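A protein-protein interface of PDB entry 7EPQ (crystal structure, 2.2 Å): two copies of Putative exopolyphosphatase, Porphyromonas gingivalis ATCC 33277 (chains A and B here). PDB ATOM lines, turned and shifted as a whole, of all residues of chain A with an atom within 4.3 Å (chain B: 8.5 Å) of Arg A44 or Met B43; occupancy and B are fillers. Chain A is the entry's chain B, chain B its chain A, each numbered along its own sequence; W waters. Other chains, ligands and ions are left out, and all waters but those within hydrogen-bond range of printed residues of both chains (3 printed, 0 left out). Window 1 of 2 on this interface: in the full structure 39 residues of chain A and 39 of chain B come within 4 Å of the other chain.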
ATOM      1  N   ASN A  19      -6.433   5.949  -7.349  1.00  0.00           N
ATOM      2  CA  ASN A  19      -6.557   7.293  -6.802  1.00  0.00           C
ATOM      3  C   ASN A  19      -5.202   7.957  -6.859  1.00  0.00           C
ATOM      4  O   ASN A  19      -4.880   8.633  -7.852  1.00  0.00           O
ATOM      5  CB  ASN A  19      -7.172   7.250  -5.394  1.00  0.00           C
ATOM      6  CG  ASN A  19      -7.398   8.645  -4.829  1.00  0.00           C
ATOM      7  OD1 ASN A  19      -7.623   9.585  -5.582  1.00  0.00           O
ATOM      8  ND2 ASN A  19      -7.313   8.789  -3.505  1.00  0.00           N
ATOM      9  N   ALA A  20      -4.347   7.811  -5.854  1.00  0.00           N
ATOM     10  CA  ALA A  20      -3.022   8.420  -5.919  1.00  0.00           C
ATOM     11  C   ALA A  20      -2.018   7.529  -6.660  1.00  0.00           C
ATOM     12  O   ALA A  20      -2.156   6.306  -6.719  1.00  0.00           O
ATOM     13  CB  ALA A  20      -2.498   8.717  -4.518  1.00  0.00           C
ATOM     14  N   VAL A  21      -0.991   8.169  -7.214  1.00  0.00           N
ATOM     15  CA  VAL A  21       0.131   7.501  -7.864  1.00  0.00           C
ATOM     16  C   VAL A  21       1.378   7.806  -7.033  1.00  0.00           C
ATOM     17  O   VAL A  21       1.756   8.976  -6.868  1.00  0.00           O
ATOM     18  CB  VAL A  21       0.303   7.960  -9.328  1.00  0.00           C
ATOM     19  CG1 VAL A  21       1.498   7.286  -9.990  1.00  0.00           C
ATOM     20  CG2 VAL A  21      -0.942   7.668 -10.138  1.00  0.00           C
ATOM     21  N   ARG A  22       2.022   6.758  -6.522  1.00  0.00           N
ATOM     22  CA  ARG A  22       3.024   6.899  -5.482  1.00  0.00           C
ATOM     23  C   ARG A  22       4.422   6.537  -5.962  1.00  0.00           C
ATOM     24  O   ARG A  22       4.612   5.682  -6.833  1.00  0.00           O
ATOM     25  CB  ARG A  22       2.686   6.022  -4.271  1.00  0.00           C
ATOM     26  CG  ARG A  22       1.425   6.406  -3.531  1.00  0.00           C
ATOM     27  CD  ARG A  22       1.196   5.460  -2.351  1.00  0.00           C
ATOM     28  NE  ARG A  22      -0.054   5.760  -1.672  1.00  0.00           N
ATOM     29  CZ  ARG A  22      -0.223   5.750  -0.354  1.00  0.00           C
ATOM     30  NH1 ARG A  22       0.789   5.448   0.457  1.00  0.00           N
ATOM     31  NH2 ARG A  22      -1.414   6.044   0.154  1.00  0.00           N
ATOM     32  N   MET A  43       6.278   9.859  -2.076  1.00  0.00           N
ATOM     33  CA  MET A  43       5.570  10.895  -2.800  1.00  0.00           C
ATOM     34  C   MET A  43       4.223  10.337  -3.215  1.00  0.00           C
ATOM     35  O   MET A  43       4.112   9.168  -3.595  1.00  0.00           O
ATOM     36  CB  MET A  43       6.365  11.363  -4.021  1.00  0.00           C
ATOM     37  CG  MET A  43       7.708  12.012  -3.644  1.00  0.00           C
ATOM     38  SD  MET A  43       8.648  12.626  -5.071  1.00  0.00           S
ATOM     39  CE  MET A  43       9.376  14.109  -4.390  1.00  0.00           C
ATOM     40  N   ARG A  44       3.202  11.179  -3.137  1.00  0.00           N
ATOM     41  CA  ARG A  44       1.836  10.767  -3.398  1.00  0.00           C
ATOM     42  C   ARG A  44       1.161  11.846  -4.225  1.00  0.00           C
ATOM     43  O   ARG A  44       1.004  12.961  -3.739  1.00  0.00           O
ATOM     44  CB  ARG A  44       1.094  10.559  -2.076  1.00  0.00           C
ATOM     45  CG  ARG A  44      -0.326  10.166  -2.270  1.00  0.00           C
ATOM     46  CD  ARG A  44      -1.053   9.959  -0.955  1.00  0.00           C
ATOM     47  NE  ARG A  44      -2.465   9.752  -1.224  1.00  0.00           N
ATOM     48  CZ  ARG A  44      -3.306  10.721  -1.570  1.00  0.00           C
ATOM     49  NH1 ARG A  44      -2.878  11.978  -1.676  1.00  0.00           N
ATOM     50  NH2 ARG A  44      -4.578  10.429  -1.817  1.00  0.00           N
ATOM     51  N   VAL A  45       0.757  11.532  -5.461  1.00  0.00           N
ATOM     52  CA  VAL A  45       0.122  12.504  -6.345  1.00  0.00           C
ATOM     53  C   VAL A  45      -1.205  11.972  -6.873  1.00  0.00           C
ATOM     54  O   VAL A  45      -1.234  10.917  -7.516  1.00  0.00           O
ATOM     55  CB  VAL A  45       1.024  12.915  -7.518  1.00  0.00           C
ATOM     56  CG1 VAL A  45       0.291  13.907  -8.405  1.00  0.00           C
ATOM     57  CG2 VAL A  45       2.328  13.509  -7.010  1.00  0.00           C
ATOM     58  N   PRO A  46      -2.335  12.665  -6.640  1.00  0.00           N
ATOM     59  CA  PRO A  46      -3.676  12.133  -7.002  1.00  0.00           C
ATOM     60  C   PRO A  46      -4.122  12.328  -8.448  1.00  0.00           C
ATOM     61  O   PRO A  46      -4.982  13.149  -8.793  1.00  0.00           O
ATOM     62  CB  PRO A  46      -4.602  12.900  -6.058  1.00  0.00           C
ATOM     63  CG  PRO A  46      -3.905  14.210  -5.827  1.00  0.00           C
ATOM     64  CD  PRO A  46      -2.428  13.884  -5.817  1.00  0.00           C
ATOM     65  N   TYR A  74       9.201  11.556 -11.055  1.00  0.00           N
ATOM     66  CA  TYR A  74       9.669  10.406 -10.275  1.00  0.00           C
ATOM     67  C   TYR A  74      10.989   9.869 -10.827  1.00  0.00           C
ATOM     68  O   TYR A  74      11.859   9.427 -10.069  1.00  0.00           O
ATOM     69  CB  TYR A  74       8.599   9.299 -10.263  1.00  0.00           C
ATOM     70  CG  TYR A  74       7.382   9.592  -9.383  1.00  0.00           C
ATOM     71  CD1 TYR A  74       7.353  10.702  -8.552  1.00  0.00           C
ATOM     72  CD2 TYR A  74       6.268   8.736  -9.378  1.00  0.00           C
ATOM     73  CE1 TYR A  74       6.247  10.969  -7.754  1.00  0.00           C
ATOM     74  CE2 TYR A  74       5.150   8.998  -8.577  1.00  0.00           C
ATOM     75  CZ  TYR A  74       5.154  10.121  -7.771  1.00  0.00           C
ATOM     76  OH  TYR A  74       4.081  10.411  -6.970  1.00  0.00           O
ATOM     77  N   ASP A 259      -8.320  15.076  -2.513  1.00  0.00           N
ATOM     78  CA  ASP A 259      -8.393  13.723  -3.056  1.00  0.00           C
ATOM     79  C   ASP A 259      -8.562  12.667  -1.977  1.00  0.00           C
ATOM     80  O   ASP A 259      -8.730  11.485  -2.302  1.00  0.00           O
ATOM     81  CB  ASP A 259      -7.134  13.364  -3.829  1.00  0.00           C
ATOM     82  CG  ASP A 259      -5.927  13.242  -2.921  1.00  0.00           C
ATOM     83  OD1 ASP A 259      -5.908  13.878  -1.854  1.00  0.00           O
ATOM     84  OD2 ASP A 259      -5.036  12.426  -3.212  1.00  0.00           O
ATOM     85  N   ARG A 260      -8.446  13.048  -0.714  1.00  0.00           N
ATOM     86  CA  ARG A 260      -8.657  12.128   0.388  1.00  0.00           C
ATOM     87  C   ARG A 260     -10.026  12.308   1.023  1.00  0.00           C
ATOM     88  O   ARG A 260     -10.615  11.324   1.489  1.00  0.00           O
ATOM     89  CB  ARG A 260      -7.556  12.332   1.427  1.00  0.00           C
ATOM     90  CG  ARG A 260      -7.853  11.792   2.802  1.00  0.00           C
ATOM     91  CD  ARG A 260      -7.557  10.314   2.848  1.00  0.00           C
ATOM     92  NE  ARG A 260      -6.199  10.039   2.385  1.00  0.00           N
ATOM     93  CZ  ARG A 260      -5.919   9.120   1.472  1.00  0.00           C
ATOM     94  NH1 ARG A 260      -6.909   8.398   0.942  1.00  0.00           N
ATOM     95  NH2 ARG A 260      -4.661   8.924   1.096  1.00  0.00           N
ATOM     96  N   ALA B  13       4.435  26.841  -3.412  1.00  0.00           N
ATOM     97  CA  ALA B  13       5.618  27.375  -2.764  1.00  0.00           C
ATOM     98  C   ALA B  13       6.714  26.323  -2.792  1.00  0.00           C
ATOM     99  O   ALA B  13       6.455  25.134  -2.559  1.00  0.00           O
ATOM    100  CB  ALA B  13       5.318  27.772  -1.319  1.00  0.00           C
ATOM    101  N   ILE B  14       7.942  26.754  -3.059  1.00  0.00           N
ATOM    102  CA  ILE B  14       9.099  25.870  -2.962  1.00  0.00           C
ATOM    103  C   ILE B  14      10.004  26.439  -1.886  1.00  0.00           C
ATOM    104  O   ILE B  14      10.446  27.591  -1.986  1.00  0.00           O
ATOM    105  CB  ILE B  14       9.839  25.717  -4.299  1.00  0.00           C
ATOM    106  CG1 ILE B  14       9.010  24.883  -5.285  1.00  0.00           C
ATOM    107  CG2 ILE B  14      11.170  25.088  -4.061  1.00  0.00           C
ATOM    108  CD1 ILE B  14       9.406  25.065  -6.754  1.00  0.00           C
ATOM    109  N   ASP B  15      10.246  25.648  -0.843  1.00  0.00           N
ATOM    110  CA  ASP B  15      10.999  26.070   0.337  1.00  0.00           C
ATOM    111  C   ASP B  15      12.325  25.324   0.304  1.00  0.00           C
ATOM    112  O   ASP B  15      12.379  24.118   0.563  1.00  0.00           O
ATOM    113  CB  ASP B  15      10.206  25.773   1.611  1.00  0.00           C
ATOM    114  CG  ASP B  15      11.004  26.015   2.893  1.00  0.00           C
ATOM    115  OD1 ASP B  15      12.099  26.611   2.854  1.00  0.00           O
ATOM    116  OD2 ASP B  15      10.503  25.622   3.972  1.00  0.00           O
ATOM    117  N   ALA B  20      15.580  19.418   4.442  1.00  0.00           N
ATOM    118  CA  ALA B  20      14.766  19.059   3.291  1.00  0.00           C
ATOM    119  C   ALA B  20      14.415  20.286   2.439  1.00  0.00           C
ATOM    120  O   ALA B  20      14.452  21.435   2.891  1.00  0.00           O
ATOM    121  CB  ALA B  20      13.489  18.356   3.732  1.00  0.00           C
ATOM    122  N   VAL B  21      14.076  20.016   1.180  1.00  0.00           N
ATOM    123  CA  VAL B  21      13.594  21.019   0.232  1.00  0.00           C
ATOM    124  C   VAL B  21      12.151  20.639  -0.123  1.00  0.00           C
ATOM    125  O   VAL B  21      11.885  19.511  -0.560  1.00  0.00           O
ATOM    126  CB  VAL B  21      14.502  21.094  -1.013  1.00  0.00           C
ATOM    127  CG1 VAL B  21      13.891  21.956  -2.091  1.00  0.00           C
ATOM    128  CG2 VAL B  21      15.911  21.613  -0.662  1.00  0.00           C
ATOM    129  N   ARG B  22      11.221  21.563   0.087  1.00  0.00           N
ATOM    130  CA  ARG B  22       9.797  21.272   0.037  1.00  0.00           C
ATOM    131  C   ARG B  22       9.099  21.944  -1.130  1.00  0.00           C
ATOM    132  O   ARG B  22       9.445  23.053  -1.537  1.00  0.00           O
ATOM    133  CB  ARG B  22       9.088  21.712   1.318  1.00  0.00           C
ATOM    134  CG  ARG B  22       9.547  20.976   2.543  1.00  0.00           C
ATOM    135  CD  ARG B  22       9.094  21.677   3.794  1.00  0.00           C
ATOM    136  NE  ARG B  22       9.596  20.953   4.954  1.00  0.00           N
ATOM    137  CZ  ARG B  22       8.813  20.438   5.885  1.00  0.00           C
ATOM    138  NH1 ARG B  22       7.489  20.584   5.779  1.00  0.00           N
ATOM    139  NH2 ARG B  22       9.354  19.779   6.907  1.00  0.00           N
ATOM    140  N   LEU B  23       8.079  21.263  -1.626  1.00  0.00           N
ATOM    141  CA  LEU B  23       7.069  21.836  -2.498  1.00  0.00           C
ATOM    142  C   LEU B  23       5.738  21.774  -1.770  1.00  0.00           C
ATOM    143  O   LEU B  23       5.376  20.724  -1.218  1.00  0.00           O
ATOM    144  CB  LEU B  23       6.988  21.076  -3.821  1.00  0.00           C
ATOM    145  CG  LEU B  23       5.770  21.406  -4.675  1.00  0.00           C
ATOM    146  CD1 LEU B  23       5.879  22.830  -5.217  1.00  0.00           C
ATOM    147  CD2 LEU B  23       5.643  20.381  -5.803  1.00  0.00           C
ATOM    148  N   LEU B  24       5.010  22.889  -1.761  1.00  0.00           N
ATOM    149  CA  LEU B  24       3.663  22.910  -1.203  1.00  0.00           C
ATOM    150  C   LEU B  24       2.703  23.522  -2.207  1.00  0.00           C
ATOM    151  O   LEU B  24       2.953  24.616  -2.730  1.00  0.00           O
ATOM    152  CB  LEU B  24       3.620  23.692   0.108  1.00  0.00           C
ATOM    153  CG  LEU B  24       2.253  23.849   0.758  1.00  0.00           C
ATOM    154  CD1 LEU B  24       1.840  22.505   1.313  1.00  0.00           C
ATOM    155  CD2 LEU B  24       2.296  24.918   1.867  1.00  0.00           C
ATOM    156  N   ILE B  25       1.593  22.831  -2.453  1.00  0.00           N
ATOM    157  CA  ILE B  25       0.524  23.340  -3.298  1.00  0.00           C
ATOM    158  C   ILE B  25      -0.758  23.391  -2.480  1.00  0.00           C
ATOM    159  O   ILE B  25      -1.073  22.461  -1.724  1.00  0.00           O
ATOM    160  CB  ILE B  25       0.331  22.493  -4.572  1.00  0.00           C
ATOM    161  CG1 ILE B  25       1.663  22.348  -5.325  1.00  0.00           C
ATOM    162  CG2 ILE B  25      -0.758  23.113  -5.474  1.00  0.00           C
ATOM    163  CD1 ILE B  25       1.549  21.693  -6.719  1.00  0.00           C
ATOM    164  N   LYS B  39      -4.270  22.805   1.786  1.00  0.00           N
ATOM    165  CA  LYS B  39      -3.160  22.028   1.248  1.00  0.00           C
ATOM    166  C   LYS B  39      -3.666  20.871   0.387  1.00  0.00           C
ATOM    167  O   LYS B  39      -4.545  20.111   0.801  1.00  0.00           O
ATOM    168  CB  LYS B  39      -2.304  21.497   2.399  1.00  0.00           C
ATOM    169  CG  LYS B  39      -1.236  20.526   1.955  1.00  0.00           C
ATOM    170  CD  LYS B  39      -0.266  20.214   3.098  1.00  0.00           C
ATOM    171  CE  LYS B  39      -0.945  19.408   4.191  1.00  0.00           C
ATOM    172  NZ  LYS B  39       0.001  19.067   5.296  1.00  0.00           N
ATOM    173  N   VAL B  40      -3.125  20.734  -0.824  1.00  0.00           N
ATOM    174  CA  VAL B  40      -3.500  19.614  -1.678  1.00  0.00           C
ATOM    175  C   VAL B  40      -2.335  18.678  -1.948  1.00  0.00           C
ATOM    176  O   VAL B  40      -2.570  17.510  -2.285  1.00  0.00           O
ATOM    177  CB  VAL B  40      -4.109  20.089  -3.020  1.00  0.00           C
ATOM    178  CG1 VAL B  40      -5.280  21.053  -2.798  1.00  0.00           C
ATOM    179  CG2 VAL B  40      -3.050  20.629  -3.967  1.00  0.00           C
ATOM    180  N   LEU B  41      -1.091  19.141  -1.818  1.00  0.00           N
ATOM    181  CA  LEU B  41       0.079  18.340  -2.132  1.00  0.00           C
ATOM    182  C   LEU B  41       1.254  18.883  -1.335  1.00  0.00           C
ATOM    183  O   LEU B  41       1.420  20.102  -1.248  1.00  0.00           O
ATOM    184  CB  LEU B  41       0.386  18.388  -3.626  1.00  0.00           C
ATOM    185  CG  LEU B  41       1.373  17.347  -4.130  1.00  0.00           C
ATOM    186  CD1 LEU B  41       0.652  16.005  -4.297  1.00  0.00           C
ATOM    187  CD2 LEU B  41       1.981  17.806  -5.432  1.00  0.00           C
ATOM    188  N   ILE B  42       2.054  17.983  -0.749  1.00  0.00           N
ATOM    189  CA  ILE B  42       3.266  18.361  -0.027  1.00  0.00           C
ATOM    190  C   ILE B  42       4.367  17.351  -0.356  1.00  0.00           C
ATOM    191  O   ILE B  42       4.154  16.134  -0.295  1.00  0.00           O
ATOM    192  CB  ILE B  42       3.023  18.474   1.498  1.00  0.00           C
ATOM    193  CG1 ILE B  42       4.317  18.809   2.272  1.00  0.00           C
ATOM    194  CG2 ILE B  42       2.423  17.198   2.068  1.00  0.00           C
ATOM    195  CD1 ILE B  42       4.906  20.235   2.072  1.00  0.00           C
ATOM    196  N   MET B  43       5.532  17.858  -0.748  1.00  0.00           N
ATOM    197  CA  MET B  43       6.714  17.047  -1.008  1.00  0.00           C
ATOM    198  C   MET B  43       7.878  17.547  -0.171  1.00  0.00           C
ATOM    199  O   MET B  43       8.049  18.756   0.024  1.00  0.00           O
ATOM    200  CB  MET B  43       7.120  17.061  -2.482  1.00  0.00           C
ATOM    201  CG  MET B  43       5.971  16.795  -3.420  1.00  0.00           C
ATOM    202  SD  MET B  43       5.831  15.018  -3.497  1.00  0.00           S
ATOM    203  CE  MET B  43       4.268  14.833  -4.364  1.00  0.00           C
ATOM    204  N   ARG B  44       8.692  16.606   0.278  1.00  0.00           N
ATOM    205  CA  ARG B  44       9.784  16.877   1.197  1.00  0.00           C
ATOM    206  C   ARG B  44      10.960  15.997   0.784  1.00  0.00           C
ATOM    207  O   ARG B  44      10.910  14.780   0.975  1.00  0.00           O
ATOM    208  CB  ARG B  44       9.343  16.583   2.631  1.00  0.00           C
ATOM    209  CG  ARG B  44      10.329  17.057   3.640  1.00  0.00           C
ATOM    210  CD  ARG B  44      10.118  16.469   5.013  1.00  0.00           C
ATOM    211  NE  ARG B  44      11.337  16.590   5.807  1.00  0.00           N
ATOM    212  CZ  ARG B  44      12.291  15.666   5.851  1.00  0.00           C
ATOM    213  NH1 ARG B  44      12.174  14.536   5.158  1.00  0.00           N
ATOM    214  NH2 ARG B  44      13.365  15.870   6.600  1.00  0.00           N
ATOM    215  N   VAL B  45      12.005  16.585   0.210  1.00  0.00           N
ATOM    216  CA  VAL B  45      13.152  15.832  -0.290  1.00  0.00           C
ATOM    217  C   VAL B  45      14.408  16.307   0.434  1.00  0.00           C
ATOM    218  O   VAL B  45      14.752  17.490   0.359  1.00  0.00           O
ATOM    219  CB  VAL B  45      13.321  15.972  -1.811  1.00  0.00           C
ATOM    220  CG1 VAL B  45      14.478  15.099  -2.300  1.00  0.00           C
ATOM    221  CG2 VAL B  45      12.021  15.603  -2.519  1.00  0.00           C
ATOM    222  N   PRO B  46      15.132  15.420   1.130  1.00  0.00           N
ATOM    223  CA  PRO B  46      16.265  15.782   2.024  1.00  0.00           C
ATOM    224  C   PRO B  46      17.600  16.038   1.332  1.00  0.00           C
ATOM    225  O   PRO B  46      18.578  15.304   1.511  1.00  0.00           O
ATOM    226  CB  PRO B  46      16.349  14.562   2.941  1.00  0.00           C
ATOM    227  CG  PRO B  46      15.881  13.420   2.097  1.00  0.00           C
ATOM    228  CD  PRO B  46      14.785  13.988   1.225  1.00  0.00           C
ATOM    229  N   LEU B  70      15.678  18.043  -8.761  1.00  0.00           N
ATOM    230  CA  LEU B  70      14.523  18.280  -7.908  1.00  0.00           C
ATOM    231  C   LEU B  70      13.660  19.396  -8.465  1.00  0.00           C
ATOM    232  O   LEU B  70      12.425  19.289  -8.483  1.00  0.00           O
ATOM    233  CB  LEU B  70      14.973  18.634  -6.494  1.00  0.00           C
ATOM    234  CG  LEU B  70      13.824  18.758  -5.476  1.00  0.00           C
ATOM    235  CD1 LEU B  70      13.024  17.460  -5.457  1.00  0.00           C
ATOM    236  CD2 LEU B  70      14.385  19.067  -4.101  1.00  0.00           C
ATOM    237  N   ALA B  73      11.554  18.122 -11.150  1.00  0.00           N
ATOM    238  CA  ALA B  73      10.441  17.336 -10.629  1.00  0.00           C
ATOM    239  C   ALA B  73       9.342  18.248 -10.091  1.00  0.00           C
ATOM    240  O   ALA B  73       8.168  18.099 -10.445  1.00  0.00           O
ATOM    241  CB  ALA B  73      10.938  16.362  -9.558  1.00  0.00           C
ATOM    242  N   TYR B  74       9.711  19.225  -9.264  1.00  0.00           N
ATOM    243  CA  TYR B  74       8.714  20.149  -8.719  1.00  0.00           C
ATOM    244  C   TYR B  74       8.071  20.981  -9.818  1.00  0.00           C
ATOM    245  O   TYR B  74       6.909  21.398  -9.698  1.00  0.00           O
ATOM    246  CB  TYR B  74       9.350  21.065  -7.673  1.00  0.00           C
ATOM    247  CG  TYR B  74       9.633  20.384  -6.345  1.00  0.00           C
ATOM    248  CD1 TYR B  74       9.224  19.085  -6.105  1.00  0.00           C
ATOM    249  CD2 TYR B  74      10.297  21.059  -5.325  1.00  0.00           C
ATOM    250  CE1 TYR B  74       9.476  18.462  -4.881  1.00  0.00           C
ATOM    251  CE2 TYR B  74      10.556  20.456  -4.103  1.00  0.00           C
ATOM    252  CZ  TYR B  74      10.139  19.157  -3.882  1.00  0.00           C
ATOM    253  OH  TYR B  74      10.402  18.561  -2.665  1.00  0.00           O
ATOM    254  N   MET B  77       5.305  18.862 -11.260  1.00  0.00           N
ATOM    255  CA  MET B  77       4.176  18.828 -10.343  1.00  0.00           C
ATOM    256  C   MET B  77       3.394  20.138 -10.382  1.00  0.00           C
ATOM    257  O   MET B  77       2.159  20.133 -10.353  1.00  0.00           O
ATOM    258  CB  MET B  77       4.669  18.500  -8.927  1.00  0.00           C
ATOM    259  CG  MET B  77       5.056  17.001  -8.744  1.00  0.00           C
ATOM    260  SD  MET B  77       5.829  16.596  -7.132  1.00  0.00           S
ATOM    261  CE  MET B  77       6.665  15.056  -7.556  1.00  0.00           C
ATOM    262  N   TYR B  81      -0.711  20.606 -11.651  1.00  0.00           N
ATOM    263  CA  TYR B  81      -1.765  21.342 -10.969  1.00  0.00           C
ATOM    264  C   TYR B  81      -2.077  22.690 -11.614  1.00  0.00           C
ATOM    265  O   TYR B  81      -2.912  23.428 -11.082  1.00  0.00           O
ATOM    266  CB  TYR B  81      -1.394  21.540  -9.495  1.00  0.00           C
ATOM    267  CG  TYR B  81      -1.732  20.342  -8.665  1.00  0.00           C
ATOM    268  CD1 TYR B  81      -0.909  19.219  -8.666  1.00  0.00           C
ATOM    269  CD2 TYR B  81      -2.891  20.312  -7.909  1.00  0.00           C
ATOM    270  CE1 TYR B  81      -1.224  18.104  -7.923  1.00  0.00           C
ATOM    271  CE2 TYR B  81      -3.214  19.200  -7.149  1.00  0.00           C
ATOM    272  CZ  TYR B  81      -2.375  18.105  -7.158  1.00  0.00           C
ATOM    273  OH  TYR B  81      -2.710  17.015  -6.412  1.00  0.00           O
ATOM    274  N   ALA B 291       6.628  27.688   3.742  1.00  0.00           N
ATOM    275  CA  ALA B 291       5.870  27.459   2.515  1.00  0.00           C
ATOM    276  C   ALA B 291       4.460  28.028   2.603  1.00  0.00           C
ATOM    277  O   ALA B 291       3.962  28.633   1.647  1.00  0.00           O
ATOM    278  CB  ALA B 291       5.807  25.962   2.219  1.00  0.00           C
HETATM  279  O   HOH W   1      -5.269  16.558  -3.024  1.00  0.00           O
HETATM  280  O   HOH W   2       3.557  13.538  -1.389  1.00  0.00           O
HETATM  281  O   HOH W   3      -1.596  14.414  -2.163  1.00  0.00           O
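The backbone NH (N) of Val B21 lies within hydrogen-bond range of the backbone carbonyl oxygen (O) of Val B45, 2.7 Å away.
The backbone carbonyl oxygen (O) of Leu B23 is in hydrogen-bond range of the backbone NH (N) of Met B43, 2.9 Å away.
The backbone NH (N) of Ile B25 lies within hydrogen-bond range of the backbone carbonyl oxygen (O) of Leu B41, at 3.0 Å.
The backbone NH (N) of Val A21 is in hydrogen-bond range of the backbone carbonyl oxygen (O) of Val A45 (2.8 Å).
OD2 of Asp A259 lies within salt-bridge range of NH2 of Arg A44 (2.5 Å).
Among the printed residues, merely in contact across the chains: Pro A46 with Tyr B81 (3.1 Å), Arg A44 with Leu B41 (3.1 Å), Val A45 with Met B43 (3.5 Å), Met A43 with Met B43 (3.5 Å), Met A43 with Val B45 (3.6 Å) and Arg A44 with Met B43 (3.8 Å).
Arg A44 touches just these residues of chain B: Leu B41 (3.1 Å) and Met B43 (3.8 Å).
Printed residues of chain B within 4 Å of Val A45: Met B43.
Of the printed residues of chain B, Pro A46 touches Tyr B81.
Ala B20 touches none of the printed residues of chain A.
Val B40 touches none of the printed residues of chain A.
Of chain A, only Met A43 (3.5 Å), Arg A44 (3.8 Å) and Val A45 (3.5 Å) come within 4 Å of Met B43.
Of the printed residues of chain A, Tyr B81 touches Pro A46 (3.1 Å).
The nearest residue of chain B that does not touch Arg A44 is Val B40 (5.6 Å).
The nearest printed residue of chain A that does not touch Met B43 is Tyr A74 (5.1 Å).
The nearest printed residue of chain A that does not touch Tyr B81 is Val A45 (4.5 Å).
Of the 11 printed residues of chain A, 4 touch a printed residue of chain B.
Among the printed residues, 6 pairs touch across the chains.
Met B43 touches its own counterpart, Met A43.
Met A43 touches Val B45, and with the chains exchanged Val A45 touches Met B43.
Arg A44 touches Met B43, but with the chains exchanged Met A43 does not touch Arg B44 (5.3 Å).
Water W3 lies within hydrogen-bond range of NH1 of Arg A44 (2.8 Å) and O of Val B40 (3.2 Å).
Water W2 lies within hydrogen-bond range of O of Ile B42, N of Arg A44 and SD of Met B43.
Water W1 lies within hydrogen-bond range of the backbone carbonyl oxygen of Val B40 (3.0 Å) and the side-chain carboxylate of Asp A259 (3.0 Å).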
